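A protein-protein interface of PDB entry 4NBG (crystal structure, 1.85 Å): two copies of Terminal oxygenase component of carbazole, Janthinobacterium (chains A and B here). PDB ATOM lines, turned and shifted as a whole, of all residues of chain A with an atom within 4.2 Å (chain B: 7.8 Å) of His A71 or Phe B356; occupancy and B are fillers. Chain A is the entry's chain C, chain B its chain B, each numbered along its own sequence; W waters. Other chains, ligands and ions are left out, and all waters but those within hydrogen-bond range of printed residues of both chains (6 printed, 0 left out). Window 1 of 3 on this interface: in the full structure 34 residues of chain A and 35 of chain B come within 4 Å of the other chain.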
ATOM      1  N   CYS A  69      -3.442 -34.809  12.229  1.00  0.00           N
ATOM      2  CA  CYS A  69      -4.371 -34.125  13.121  1.00  0.00           C
ATOM      3  C   CYS A  69      -4.147 -32.614  13.053  1.00  0.00           C
ATOM      4  O   CYS A  69      -3.010 -32.150  12.990  1.00  0.00           O
ATOM      5  CB  CYS A  69      -4.168 -34.618  14.554  1.00  0.00           C
ATOM      6  SG  CYS A  69      -5.439 -34.070  15.717  1.00  0.00           S
ATOM      7  N   LEU A  70      -5.240 -31.856  13.067  1.00  0.00           N
ATOM      8  CA  LEU A  70      -5.193 -30.396  13.009  1.00  0.00           C
ATOM      9  C   LEU A  70      -4.550 -29.787  14.251  1.00  0.00           C
ATOM     10  O   LEU A  70      -3.983 -28.694  14.201  1.00  0.00           O
ATOM     11  CB  LEU A  70      -6.614 -29.830  12.889  1.00  0.00           C
ATOM     12  CG  LEU A  70      -7.463 -30.198  11.668  1.00  0.00           C
ATOM     13  CD1 LEU A  70      -8.835 -29.556  11.801  1.00  0.00           C
ATOM     14  CD2 LEU A  70      -6.783 -29.715  10.394  1.00  0.00           C
ATOM     15  N   HIS A  71      -4.652 -30.505  15.361  1.00  0.00           N
ATOM     16  CA  HIS A  71      -4.140 -30.053  16.649  1.00  0.00           C
ATOM     17  C   HIS A  71      -2.619 -29.895  16.731  1.00  0.00           C
ATOM     18  O   HIS A  71      -2.101 -28.781  16.619  1.00  0.00           O
ATOM     19  CB  HIS A  71      -4.626 -31.007  17.740  1.00  0.00           C
ATOM     20  CG  HIS A  71      -4.334 -30.538  19.130  1.00  0.00           C
ATOM     21  ND1 HIS A  71      -4.187 -31.407  20.188  1.00  0.00           N
ATOM     22  CD2 HIS A  71      -4.171 -29.293  19.639  1.00  0.00           C
ATOM     23  CE1 HIS A  71      -3.940 -30.717  21.289  1.00  0.00           C
ATOM     24  NE2 HIS A  71      -3.926 -29.432  20.982  1.00  0.00           N
ATOM     25  N   ARG A  72      -1.910 -31.003  16.936  1.00  0.00           N
ATOM     26  CA  ARG A  72      -0.456 -30.960  17.049  1.00  0.00           C
ATOM     27  C   ARG A  72       0.278 -31.635  15.887  1.00  0.00           C
ATOM     28  O   ARG A  72       1.442 -32.010  16.011  1.00  0.00           O
ATOM     29  CB  ARG A  72      -0.013 -31.579  18.378  1.00  0.00           C
ATOM     30  CG  ARG A  72      -0.620 -30.901  19.614  1.00  0.00           C
ATOM     31  CD  ARG A  72      -0.337 -29.399  19.654  1.00  0.00           C
ATOM     32  NE  ARG A  72       1.094 -29.093  19.725  1.00  0.00           N
ATOM     33  CZ  ARG A  72       1.843 -29.218  20.818  1.00  0.00           C
ATOM     34  NH1 ARG A  72       1.307 -29.640  21.956  1.00  0.00           N
ATOM     35  NH2 ARG A  72       3.138 -28.930  20.770  1.00  0.00           N
ATOM     36  N   GLY A  73      -0.425 -31.804  14.770  1.00  0.00           N
ATOM     37  CA  GLY A  73       0.165 -32.376  13.569  1.00  0.00           C
ATOM     38  C   GLY A  73       0.709 -33.792  13.548  1.00  0.00           C
ATOM     39  O   GLY A  73       1.604 -34.095  12.750  1.00  0.00           O
ATOM     40  N   HIS A  93      -5.242 -36.382  21.751  1.00  0.00           N
ATOM     41  CA  HIS A  93      -6.175 -35.642  22.600  1.00  0.00           C
ATOM     42  C   HIS A  93      -7.628 -35.879  22.196  1.00  0.00           C
ATOM     43  O   HIS A  93      -8.512 -35.074  22.489  1.00  0.00           O
ATOM     44  CB  HIS A  93      -5.854 -34.147  22.563  1.00  0.00           C
ATOM     45  CG  HIS A  93      -4.406 -33.840  22.788  1.00  0.00           C
ATOM     46  ND1 HIS A  93      -3.476 -33.861  21.771  1.00  0.00           N
ATOM     47  CD2 HIS A  93      -3.725 -33.519  23.914  1.00  0.00           C
ATOM     48  CE1 HIS A  93      -2.285 -33.563  22.261  1.00  0.00           C
ATOM     49  NE2 HIS A  93      -2.408 -33.353  23.559  1.00  0.00           N
ATOM     50  N   TRP A  95      -9.374 -35.635  19.367  1.00  0.00           N
ATOM     51  CA  TRP A  95     -10.123 -34.798  18.440  1.00  0.00           C
ATOM     52  C   TRP A  95     -10.722 -35.818  17.474  1.00  0.00           C
ATOM     53  O   TRP A  95     -10.006 -36.669  16.947  1.00  0.00           O
ATOM     54  CB  TRP A  95      -9.195 -33.843  17.688  1.00  0.00           C
ATOM     55  CG  TRP A  95      -8.812 -32.624  18.478  1.00  0.00           C
ATOM     56  CD1 TRP A  95      -8.621 -32.548  19.827  1.00  0.00           C
ATOM     57  CD2 TRP A  95      -8.523 -31.323  17.957  1.00  0.00           C
ATOM     58  NE1 TRP A  95      -8.228 -31.279  20.182  1.00  0.00           N
ATOM     59  CE2 TRP A  95      -8.159 -30.505  19.053  1.00  0.00           C
ATOM     60  CE3 TRP A  95      -8.534 -30.765  16.671  1.00  0.00           C
ATOM     61  CZ2 TRP A  95      -7.806 -29.159  18.900  1.00  0.00           C
ATOM     62  CZ3 TRP A  95      -8.185 -29.424  16.519  1.00  0.00           C
ATOM     63  CH2 TRP A  95      -7.824 -28.637  17.631  1.00  0.00           C
ATOM     64  N   ILE A 107     -14.683 -33.921  20.595  1.00  0.00           N
ATOM     65  CA  ILE A 107     -13.364 -33.933  21.222  1.00  0.00           C
ATOM     66  C   ILE A 107     -13.582 -34.558  22.593  1.00  0.00           C
ATOM     67  O   ILE A 107     -14.095 -33.911  23.505  1.00  0.00           O
ATOM     68  CB  ILE A 107     -12.773 -32.515  21.395  1.00  0.00           C
ATOM     69  CG1 ILE A 107     -12.576 -31.853  20.026  1.00  0.00           C
ATOM     70  CG2 ILE A 107     -11.438 -32.608  22.131  1.00  0.00           C
ATOM     71  CD1 ILE A 107     -11.946 -30.466  20.090  1.00  0.00           C
ATOM     72  N   THR A 109     -11.576 -35.307  25.022  1.00  0.00           N
ATOM     73  CA  THR A 109     -10.863 -34.707  26.149  1.00  0.00           C
ATOM     74  C   THR A 109     -11.480 -33.395  26.620  1.00  0.00           C
ATOM     75  O   THR A 109     -11.134 -32.892  27.688  1.00  0.00           O
ATOM     76  CB  THR A 109      -9.384 -34.451  25.807  1.00  0.00           C
ATOM     77  OG1 THR A 109      -9.298 -33.624  24.642  1.00  0.00           O
ATOM     78  CG2 THR A 109      -8.660 -35.768  25.563  1.00  0.00           C
ATOM     79  N   ASN A 110     -12.383 -32.833  25.823  1.00  0.00           N
ATOM     80  CA  ASN A 110     -13.048 -31.587  26.197  1.00  0.00           C
ATOM     81  C   ASN A 110     -14.300 -31.362  25.367  1.00  0.00           C
ATOM     82  O   ASN A 110     -14.275 -30.657  24.358  1.00  0.00           O
ATOM     83  CB  ASN A 110     -12.111 -30.387  26.039  1.00  0.00           C
ATOM     84  CG  ASN A 110     -12.771 -29.085  26.456  1.00  0.00           C
ATOM     85  OD1 ASN A 110     -13.847 -29.088  27.062  1.00  0.00           O
ATOM     86  ND2 ASN A 110     -12.129 -27.965  26.144  1.00  0.00           N
ATOM     87  N   SER A 113     -15.196 -27.742  24.232  1.00  0.00           N
ATOM     88  CA  SER A 113     -14.283 -26.972  23.392  1.00  0.00           C
ATOM     89  C   SER A 113     -14.969 -26.173  22.290  1.00  0.00           C
ATOM     90  O   SER A 113     -15.854 -26.674  21.597  1.00  0.00           O
ATOM     91  CB  SER A 113     -13.243 -27.898  22.758  1.00  0.00           C
ATOM     92  OG  SER A 113     -12.337 -27.147  21.967  1.00  0.00           O
ATOM     93  N   GLN A 115     -13.677 -25.385  19.638  1.00  0.00           N
ATOM     94  CA  GLN A 115     -13.173 -25.864  18.352  1.00  0.00           C
ATOM     95  C   GLN A 115     -14.143 -26.835  17.689  1.00  0.00           C
ATOM     96  O   GLN A 115     -14.170 -26.960  16.468  1.00  0.00           O
ATOM     97  CB  GLN A 115     -11.815 -26.551  18.532  1.00  0.00           C
ATOM     98  CG  GLN A 115     -10.701 -25.612  18.964  1.00  0.00           C
ATOM     99  CD  GLN A 115     -10.344 -24.605  17.888  1.00  0.00           C
ATOM    100  OE1 GLN A 115     -11.163 -24.277  17.031  1.00  0.00           O
ATOM    101  NE2 GLN A 115      -9.118 -24.097  17.937  1.00  0.00           N
ATOM    102  N   ASP B 180       1.187 -31.190  29.167  1.00  0.00           N
ATOM    103  CA  ASP B 180      -0.075 -31.172  28.422  1.00  0.00           C
ATOM    104  C   ASP B 180      -1.211 -31.763  29.264  1.00  0.00           C
ATOM    105  O   ASP B 180      -1.248 -32.967  29.499  1.00  0.00           O
ATOM    106  CB  ASP B 180       0.097 -32.005  27.147  1.00  0.00           C
ATOM    107  CG  ASP B 180      -1.038 -31.828  26.164  1.00  0.00           C
ATOM    108  OD1 ASP B 180      -2.205 -31.714  26.598  1.00  0.00           O
ATOM    109  OD2 ASP B 180      -0.759 -31.822  24.945  1.00  0.00           O
ATOM    110  N   PRO B 181      -2.165 -30.930  29.707  1.00  0.00           N
ATOM    111  CA  PRO B 181      -3.267 -31.453  30.525  1.00  0.00           C
ATOM    112  C   PRO B 181      -4.122 -32.531  29.855  1.00  0.00           C
ATOM    113  O   PRO B 181      -4.492 -33.522  30.488  1.00  0.00           O
ATOM    114  CB  PRO B 181      -4.089 -30.201  30.846  1.00  0.00           C
ATOM    115  CG  PRO B 181      -3.078 -29.088  30.774  1.00  0.00           C
ATOM    116  CD  PRO B 181      -2.281 -29.472  29.546  1.00  0.00           C
ATOM    117  N   SER B 182      -4.429 -32.341  28.577  1.00  0.00           N
ATOM    118  CA  SER B 182      -5.274 -33.289  27.856  1.00  0.00           C
ATOM    119  C   SER B 182      -4.603 -34.531  27.288  1.00  0.00           C
ATOM    120  O   SER B 182      -5.298 -35.416  26.790  1.00  0.00           O
ATOM    121  CB  SER B 182      -6.015 -32.576  26.725  1.00  0.00           C
ATOM    122  OG  SER B 182      -6.974 -31.675  27.237  1.00  0.00           O
ATOM    123  N   HIS B 183      -3.275 -34.616  27.356  1.00  0.00           N
ATOM    124  CA  HIS B 183      -2.595 -35.784  26.811  1.00  0.00           C
ATOM    125  C   HIS B 183      -2.827 -37.002  27.692  1.00  0.00           C
ATOM    126  O   HIS B 183      -2.444 -38.117  27.342  1.00  0.00           O
ATOM    127  CB  HIS B 183      -1.086 -35.527  26.641  1.00  0.00           C
ATOM    128  CG  HIS B 183      -0.249 -35.986  27.794  1.00  0.00           C
ATOM    129  ND1 HIS B 183      -0.149 -35.279  28.973  1.00  0.00           N
ATOM    130  CD2 HIS B 183       0.528 -37.083  27.947  1.00  0.00           C
ATOM    131  CE1 HIS B 183       0.655 -35.920  29.801  1.00  0.00           C
ATOM    132  NE2 HIS B 183       1.079 -37.019  29.204  1.00  0.00           N
ATOM    133  N   PHE B 204     -10.440 -32.876  30.536  1.00  0.00           N
ATOM    134  CA  PHE B 204     -11.048 -31.874  31.400  1.00  0.00           C
ATOM    135  C   PHE B 204     -11.854 -30.846  30.627  1.00  0.00           C
ATOM    136  O   PHE B 204     -11.461 -30.422  29.543  1.00  0.00           O
ATOM    137  CB  PHE B 204      -9.965 -31.127  32.180  1.00  0.00           C
ATOM    138  CG  PHE B 204      -9.040 -32.021  32.941  1.00  0.00           C
ATOM    139  CD1 PHE B 204      -9.381 -32.480  34.209  1.00  0.00           C
ATOM    140  CD2 PHE B 204      -7.831 -32.424  32.382  1.00  0.00           C
ATOM    141  CE1 PHE B 204      -8.530 -33.330  34.912  1.00  0.00           C
ATOM    142  CE2 PHE B 204      -6.974 -33.274  33.071  1.00  0.00           C
ATOM    143  CZ  PHE B 204      -7.325 -33.729  34.341  1.00  0.00           C
ATOM    144  N   PRO B 206     -12.634 -27.286  30.880  1.00  0.00           N
ATOM    145  CA  PRO B 206     -12.164 -26.088  31.585  1.00  0.00           C
ATOM    146  C   PRO B 206     -13.250 -25.256  32.250  1.00  0.00           C
ATOM    147  O   PRO B 206     -14.410 -25.274  31.837  1.00  0.00           O
ATOM    148  CB  PRO B 206     -11.438 -25.305  30.491  1.00  0.00           C
ATOM    149  CG  PRO B 206     -10.951 -26.383  29.572  1.00  0.00           C
ATOM    150  CD  PRO B 206     -12.154 -27.288  29.487  1.00  0.00           C
ATOM    151  N   MET B 340       5.199 -36.059  17.116  1.00  0.00           N
ATOM    152  CA  MET B 340       5.114 -34.640  16.765  1.00  0.00           C
ATOM    153  C   MET B 340       6.357 -34.138  16.034  1.00  0.00           C
ATOM    154  O   MET B 340       6.383 -33.009  15.546  1.00  0.00           O
ATOM    155  CB  MET B 340       4.918 -33.775  18.018  1.00  0.00           C
ATOM    156  CG  MET B 340       3.547 -33.860  18.670  1.00  0.00           C
ATOM    157  SD  MET B 340       3.377 -32.568  19.936  1.00  0.00           S
ATOM    158  CE  MET B 340       4.329 -33.263  21.250  1.00  0.00           C
ATOM    159  N   PHE B 343       5.926 -32.661  12.247  1.00  0.00           N
ATOM    160  CA  PHE B 343       5.200 -31.399  12.178  1.00  0.00           C
ATOM    161  C   PHE B 343       6.040 -30.189  12.584  1.00  0.00           C
ATOM    162  O   PHE B 343       5.906 -29.109  12.007  1.00  0.00           O
ATOM    163  CB  PHE B 343       3.949 -31.492  13.060  1.00  0.00           C
ATOM    164  CG  PHE B 343       2.962 -30.378  12.852  1.00  0.00           C
ATOM    165  CD1 PHE B 343       2.447 -30.109  11.586  1.00  0.00           C
ATOM    166  CD2 PHE B 343       2.504 -29.632  13.937  1.00  0.00           C
ATOM    167  CE1 PHE B 343       1.484 -29.114  11.400  1.00  0.00           C
ATOM    168  CE2 PHE B 343       1.539 -28.634  13.763  1.00  0.00           C
ATOM    169  CZ  PHE B 343       1.029 -28.378  12.491  1.00  0.00           C
ATOM    170  N   TYR B 344       6.913 -30.372  13.569  1.00  0.00           N
ATOM    171  CA  TYR B 344       7.750 -29.277  14.052  1.00  0.00           C
ATOM    172  C   TYR B 344       9.178 -29.275  13.504  1.00  0.00           C
ATOM    173  O   TYR B 344       9.922 -28.316  13.715  1.00  0.00           O
ATOM    174  CB  TYR B 344       7.788 -29.309  15.581  1.00  0.00           C
ATOM    175  CG  TYR B 344       6.469 -28.921  16.207  1.00  0.00           C
ATOM    176  CD1 TYR B 344       6.155 -27.582  16.434  1.00  0.00           C
ATOM    177  CD2 TYR B 344       5.515 -29.886  16.531  1.00  0.00           C
ATOM    178  CE1 TYR B 344       4.924 -27.210  16.967  1.00  0.00           C
ATOM    179  CE2 TYR B 344       4.272 -29.524  17.066  1.00  0.00           C
ATOM    180  CZ  TYR B 344       3.988 -28.182  17.278  1.00  0.00           C
ATOM    181  OH  TYR B 344       2.765 -27.802  17.783  1.00  0.00           O
ATOM    182  N   GLY B 349       5.470 -26.127  12.377  1.00  0.00           N
ATOM    183  CA  GLY B 349       4.447 -26.505  13.336  1.00  0.00           C
ATOM    184  C   GLY B 349       4.185 -25.420  14.368  1.00  0.00           C
ATOM    185  O   GLY B 349       3.074 -25.312  14.898  1.00  0.00           O
ATOM    186  N   ASN B 352       1.567 -23.379  12.367  1.00  0.00           N
ATOM    187  CA  ASN B 352       0.353 -24.059  11.918  1.00  0.00           C
ATOM    188  C   ASN B 352      -0.468 -24.853  12.932  1.00  0.00           C
ATOM    189  O   ASN B 352      -1.594 -25.258  12.635  1.00  0.00           O
ATOM    190  CB  ASN B 352       0.695 -24.963  10.727  1.00  0.00           C
ATOM    191  CG  ASN B 352       1.141 -24.171   9.516  1.00  0.00           C
ATOM    192  OD1 ASN B 352       0.487 -23.207   9.126  1.00  0.00           O
ATOM    193  ND2 ASN B 352       2.251 -24.576   8.912  1.00  0.00           N
ATOM    194  N   GLU B 353       0.086 -25.085  14.116  1.00  0.00           N
ATOM    195  CA  GLU B 353      -0.619 -25.822  15.162  1.00  0.00           C
ATOM    196  C   GLU B 353      -1.962 -25.144  15.461  1.00  0.00           C
ATOM    197  O   GLU B 353      -2.043 -23.920  15.479  1.00  0.00           O
ATOM    198  CB  GLU B 353       0.228 -25.828  16.439  1.00  0.00           C
ATOM    199  CG  GLU B 353       0.483 -24.417  16.966  1.00  0.00           C
ATOM    200  CD  GLU B 353       1.471 -24.361  18.120  1.00  0.00           C
ATOM    201  OE1 GLU B 353       2.030 -25.413  18.495  1.00  0.00           O
ATOM    202  OE2 GLU B 353       1.687 -23.250  18.649  1.00  0.00           O
ATOM    203  N   ILE B 354      -3.010 -25.934  15.679  1.00  0.00           N
ATOM    204  CA  ILE B 354      -4.325 -25.388  16.017  1.00  0.00           C
ATOM    205  C   ILE B 354      -4.602 -25.820  17.456  1.00  0.00           C
ATOM    206  O   ILE B 354      -4.981 -26.960  17.715  1.00  0.00           O
ATOM    207  CB  ILE B 354      -5.424 -25.920  15.063  1.00  0.00           C
ATOM    208  CG1 ILE B 354      -5.172 -25.384  13.646  1.00  0.00           C
ATOM    209  CG2 ILE B 354      -6.806 -25.491  15.560  1.00  0.00           C
ATOM    210  CD1 ILE B 354      -6.166 -25.862  12.600  1.00  0.00           C
ATOM    211  N   LEU B 355      -4.391 -24.900  18.392  1.00  0.00           N
ATOM    212  CA  LEU B 355      -4.559 -25.193  19.812  1.00  0.00           C
ATOM    213  C   LEU B 355      -5.997 -25.106  20.303  1.00  0.00           C
ATOM    214  O   LEU B 355      -6.829 -24.445  19.689  1.00  0.00           O
ATOM    215  CB  LEU B 355      -3.701 -24.224  20.641  1.00  0.00           C
ATOM    216  CG  LEU B 355      -2.242 -24.050  20.197  1.00  0.00           C
ATOM    217  CD1 LEU B 355      -1.554 -22.994  21.058  1.00  0.00           C
ATOM    218  CD2 LEU B 355      -1.522 -25.382  20.301  1.00  0.00           C
ATOM    219  N   PHE B 356      -6.288 -25.802  21.398  1.00  0.00           N
ATOM    220  CA  PHE B 356      -7.615 -25.719  21.992  1.00  0.00           C
ATOM    221  C   PHE B 356      -7.447 -25.350  23.465  1.00  0.00           C
ATOM    222  O   PHE B 356      -6.319 -25.201  23.939  1.00  0.00           O
ATOM    223  CB  PHE B 356      -8.453 -26.997  21.748  1.00  0.00           C
ATOM    224  CG  PHE B 356      -8.085 -28.195  22.585  1.00  0.00           C
ATOM    225  CD1 PHE B 356      -6.761 -28.528  22.856  1.00  0.00           C
ATOM    226  CD2 PHE B 356      -9.090 -29.068  23.006  1.00  0.00           C
ATOM    227  CE1 PHE B 356      -6.442 -29.715  23.525  1.00  0.00           C
ATOM    228  CE2 PHE B 356      -8.784 -30.254  23.673  1.00  0.00           C
ATOM    229  CZ  PHE B 356      -7.457 -30.582  23.933  1.00  0.00           C
ATOM    230  N   GLU B 357      -8.556 -25.174  24.176  1.00  0.00           N
ATOM    231  CA  GLU B 357      -8.527 -24.732  25.571  1.00  0.00           C
ATOM    232  C   GLU B 357      -7.427 -25.176  26.544  1.00  0.00           C
ATOM    233  O   GLU B 357      -6.751 -24.324  27.131  1.00  0.00           O
ATOM    234  CB  GLU B 357      -9.893 -24.986  26.223  1.00  0.00           C
ATOM    235  CG  GLU B 357     -11.029 -24.131  25.659  1.00  0.00           C
ATOM    236  CD  GLU B 357     -11.528 -24.613  24.306  1.00  0.00           C
ATOM    237  OE1 GLU B 357     -11.137 -25.719  23.881  1.00  0.00           O
ATOM    238  OE2 GLU B 357     -12.326 -23.888  23.673  1.00  0.00           O
ATOM    239  N   SER B 358      -7.237 -26.478  26.734  1.00  0.00           N
ATOM    240  CA  SER B 358      -6.228 -26.945  27.684  1.00  0.00           C
ATOM    241  C   SER B 358      -4.781 -26.567  27.358  1.00  0.00           C
ATOM    242  O   SER B 358      -3.910 -26.632  28.231  1.00  0.00           O
ATOM    243  CB  SER B 358      -6.338 -28.463  27.885  1.00  0.00           C
ATOM    244  OG  SER B 358      -6.171 -29.178  26.673  1.00  0.00           O
ATOM    245  N   ASP B 359      -4.521 -26.153  26.122  1.00  0.00           N
ATOM    246  CA  ASP B 359      -3.168 -25.771  25.739  1.00  0.00           C
ATOM    247  C   ASP B 359      -2.783 -24.440  26.370  1.00  0.00           C
ATOM    248  O   ASP B 359      -1.690 -23.919  26.141  1.00  0.00           O
ATOM    249  CB  ASP B 359      -3.039 -25.690  24.217  1.00  0.00           C
ATOM    250  CG  ASP B 359      -3.175 -27.044  23.555  1.00  0.00           C
ATOM    251  OD1 ASP B 359      -2.646 -28.025  24.118  1.00  0.00           O
ATOM    252  OD2 ASP B 359      -3.795 -27.131  22.476  1.00  0.00           O
ATOM    253  N   GLU B 360      -3.693 -23.888  27.163  1.00  0.00           N
ATOM    254  CA  GLU B 360      -3.431 -22.632  27.843  1.00  0.00           C
ATOM    255  C   GLU B 360      -2.212 -22.867  28.732  1.00  0.00           C
ATOM    256  O   GLU B 360      -1.396 -21.970  28.936  1.00  0.00           O
ATOM    257  CB  GLU B 360      -4.635 -22.235  28.696  1.00  0.00           C
ATOM    258  CG  GLU B 360      -4.634 -20.784  29.112  1.00  0.00           C
ATOM    259  CD  GLU B 360      -4.761 -19.845  27.924  1.00  0.00           C
ATOM    260  OE1 GLU B 360      -5.826 -19.848  27.260  1.00  0.00           O
ATOM    261  OE2 GLU B 360      -3.796 -19.107  27.651  1.00  0.00           O
ATOM    262  N   ALA B 361      -2.098 -24.083  29.253  1.00  0.00           N
ATOM    263  CA  ALA B 361      -0.978 -24.455  30.111  1.00  0.00           C
ATOM    264  C   ALA B 361       0.330 -24.429  29.326  1.00  0.00           C
ATOM    265  O   ALA B 361       1.349 -23.941  29.817  1.00  0.00           O
ATOM    266  CB  ALA B 361      -1.202 -25.843  30.696  1.00  0.00           C
ATOM    267  N   ILE B 362       0.302 -24.964  28.108  1.00  0.00           N
ATOM    268  CA  ILE B 362       1.495 -24.986  27.269  1.00  0.00           C
ATOM    269  C   ILE B 362       1.909 -23.553  26.917  1.00  0.00           C
ATOM    270  O   ILE B 362       3.090 -23.214  26.965  1.00  0.00           O
ATOM    271  CB  ILE B 362       1.245 -25.819  25.983  1.00  0.00           C
ATOM    272  CG1 ILE B 362       1.086 -27.299  26.364  1.00  0.00           C
ATOM    273  CG2 ILE B 362       2.397 -25.639  24.997  1.00  0.00           C
ATOM    274  CD1 ILE B 362       0.720 -28.217  25.205  1.00  0.00           C
ATOM    275  N   VAL B 363       0.936 -22.711  26.586  1.00  0.00           N
ATOM    276  CA  VAL B 363       1.221 -21.318  26.246  1.00  0.00           C
ATOM    277  C   VAL B 363       1.887 -20.606  27.425  1.00  0.00           C
ATOM    278  O   VAL B 363       2.845 -19.854  27.243  1.00  0.00           O
ATOM    279  CB  VAL B 363      -0.072 -20.553  25.863  1.00  0.00           C
ATOM    280  CG1 VAL B 363       0.200 -19.057  25.801  1.00  0.00           C
ATOM    281  CG2 VAL B 363      -0.586 -21.046  24.514  1.00  0.00           C
HETATM  282  O   HOH W   1      -2.808 -27.665  12.017  1.00  0.00           O
HETATM  283  O   HOH W   2       4.247 -34.864  13.296  1.00  0.00           O
HETATM  284  O   HOH W   3      -9.209 -30.042  28.152  1.00  0.00           O
HETATM  285  O   HOH W   4      -9.232 -28.288  26.010  1.00  0.00           O
HETATM  286  O   HOH W   5      -1.209 -30.055  23.009  1.00  0.00           O
HETATM  287  O   HOH W   6       1.794 -31.886  23.693  1.00  0.00           O
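Among the printed residues, pairs that only touch across the chains: Trp A95 with Ile B354 (3.3 Å), Arg A72 with Phe B343 (3.3 Å), Asn A110 with Pro B206 (3.4 Å), His A71 with Phe B356 (3.5 Å), Gly A73 with Phe B343 (3.5 Å), Thr A109 with Phe B356 (3.5 Å), Asn A110 with Phe B204 (3.6 Å), Arg A72 with Ile B362 (3.6 Å), Thr A109 with Ser B182 (3.6 Å), Gln A115 with Ile B354 (3.6 Å), His A71 with Glu B353 (3.6 Å), His A93 with Ser B182 (3.6 Å), Trp A95 with Phe B356 (3.6 Å), His A93 with His B183 (3.6 Å), Gln A115 with Phe B356 (3.8 Å), Ile A107 with Phe B356 (3.9 Å) and Ser A113 with Phe B356 (3.9 Å).
Of the 22 printed residues of chain B, 15 touch a printed residue of chain A.
Hydrophobic or aromatic side chains of chain B that line the printed part of chain A: His B183, Pro B206, Met B340, Phe B343, Tyr B344, Ile B354, Phe B356 and Ile B362.
Of the 12 printed residues of chain A, 11 touch a printed residue of chain B.
Hydrophobic or aromatic side chains of chain A that line the printed part of chain B: His A71, His A93, Trp A95 and Ile A107.
The side-chain carboxylate of Asp B180 sits at hydrogen-bond distance from a ring nitrogen (NE2) of His A93, at 2.6 Å.
N of Phe B204 lies within hydrogen-bond range of O of Thr A109, at 2.9 Å.
NH2 of Arg A72 lies within hydrogen-bond range of SD of Met B340, 3.7 Å away.
OH of Tyr B344 is in hydrogen-bond range of NE of Arg A72, 2.9 Å away.
The guanidinium group of Arg A72 lies within salt-bridge range of the side-chain carboxylate of Glu B353 (3.99 Å).
The backbone carbonyl oxygen (O) of Leu A70 sits close to the backbone NH (N) of Ile B354 (3.3 Å).
N of Ile B354 sits at hydrogen-bond distance from O of His A71, at 3.1 Å.
NE2 of Gln A115 lies within hydrogen-bond range of O of Leu B355, 2.9 Å away.
OE1 of Glu B357 sits at hydrogen-bond distance from ND2 of Asn A110.
The side-chain carboxylate (OE1) of Glu B357 lies within hydrogen-bond range of the side-chain hydroxyl (OG) of Ser A113, 2.7 Å away.
OD2 of Asp B359 sits at hydrogen-bond distance from NE2 of His A71 (2.7 Å).
Printed residues of chain B within 4 Å of His A71: Glu B353 (3.6 Å), Ile B354 (3.1 Å), Phe B356 (3.5 Å) and Asp B359 (2.7 Å).
Phe B356 touches six residues of chain A.
Of the printed residues of chain A, His B183 touches His A93 (3.6 Å).
Printed residues of chain A within 4 Å of Asp B180: His A93.
Printed residues of chain A within 4 Å of Tyr B344: Arg A72 (2.9 Å).
Of the printed residues of chain A, Leu B355 touches Gln A115 (2.9 Å).
Printed residues of chain B within 4 Å of Leu A70: Ile B354.
Pro B181 touches none of the printed residues of chain A.
Cys A69 touches none of the printed residues of chain B.
The nearest residue of chain B that does not touch His A71 is Leu B355 (4.1 Å).
The nearest printed residue of chain B that does not touch Asn A110 is Phe B356 (4.1 Å).
O of Asp B180 sits at hydrogen-bond distance from ND1 of His B183, 2.6 Å away.
The side-chain hydroxyl (OG) of Ser B182 sits at hydrogen-bond distance from the side-chain hydroxyl (OG) of Ser B358 (2.7 Å).
The side-chain carboxylate (OE1) of Glu B353 lies within hydrogen-bond range of the side-chain hydroxyl (OH) of Tyr B344, 2.6 Å away.
The backbone NH of Phe B356 sits at hydrogen-bond distance from the side-chain carboxylate of Asp B359, 3.0 Å away.
The side-chain hydroxyl of Thr A109 lies within hydrogen-bond range of the backbone carbonyl oxygen of His A93 (2.7 Å).
The side-chain hydroxyl (OG) of Ser A113 lies close to the backbone NH (N) of Gln A115 (3.2 Å).
No position is printed for both chains.
Of the 28 pairs that touch across the chains among the printed residues, none has its exchanged pair printed and touching as well.
Water W5 lies within hydrogen-bond range of the side-chain carboxylate of Asp B180 (2.7 Å), the side-chain carboxylate of Asp B359 (2.7 Å), the guanidinium group of Arg A72 (2.8 Å) and a ring nitrogen (NE2) of His A71 (3.4 Å).
Water W3 lies within hydrogen-bond range of O of Phe B204, OG of Ser B182, O of Thr A109 and OG of Ser B358.
Water W1 lies within hydrogen-bond range of O of Leu A70 and O of Asn B352.
Water W4 bridges N of Ser B358 and ND2 of Asn A110.
Water W2 bridges O of Gly A73 (2.8 Å) and N of Phe B343 (3.0 Å).
Water W6 lies within hydrogen-bond range of OD2 of Asp B180 and NH1 of Arg A72.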
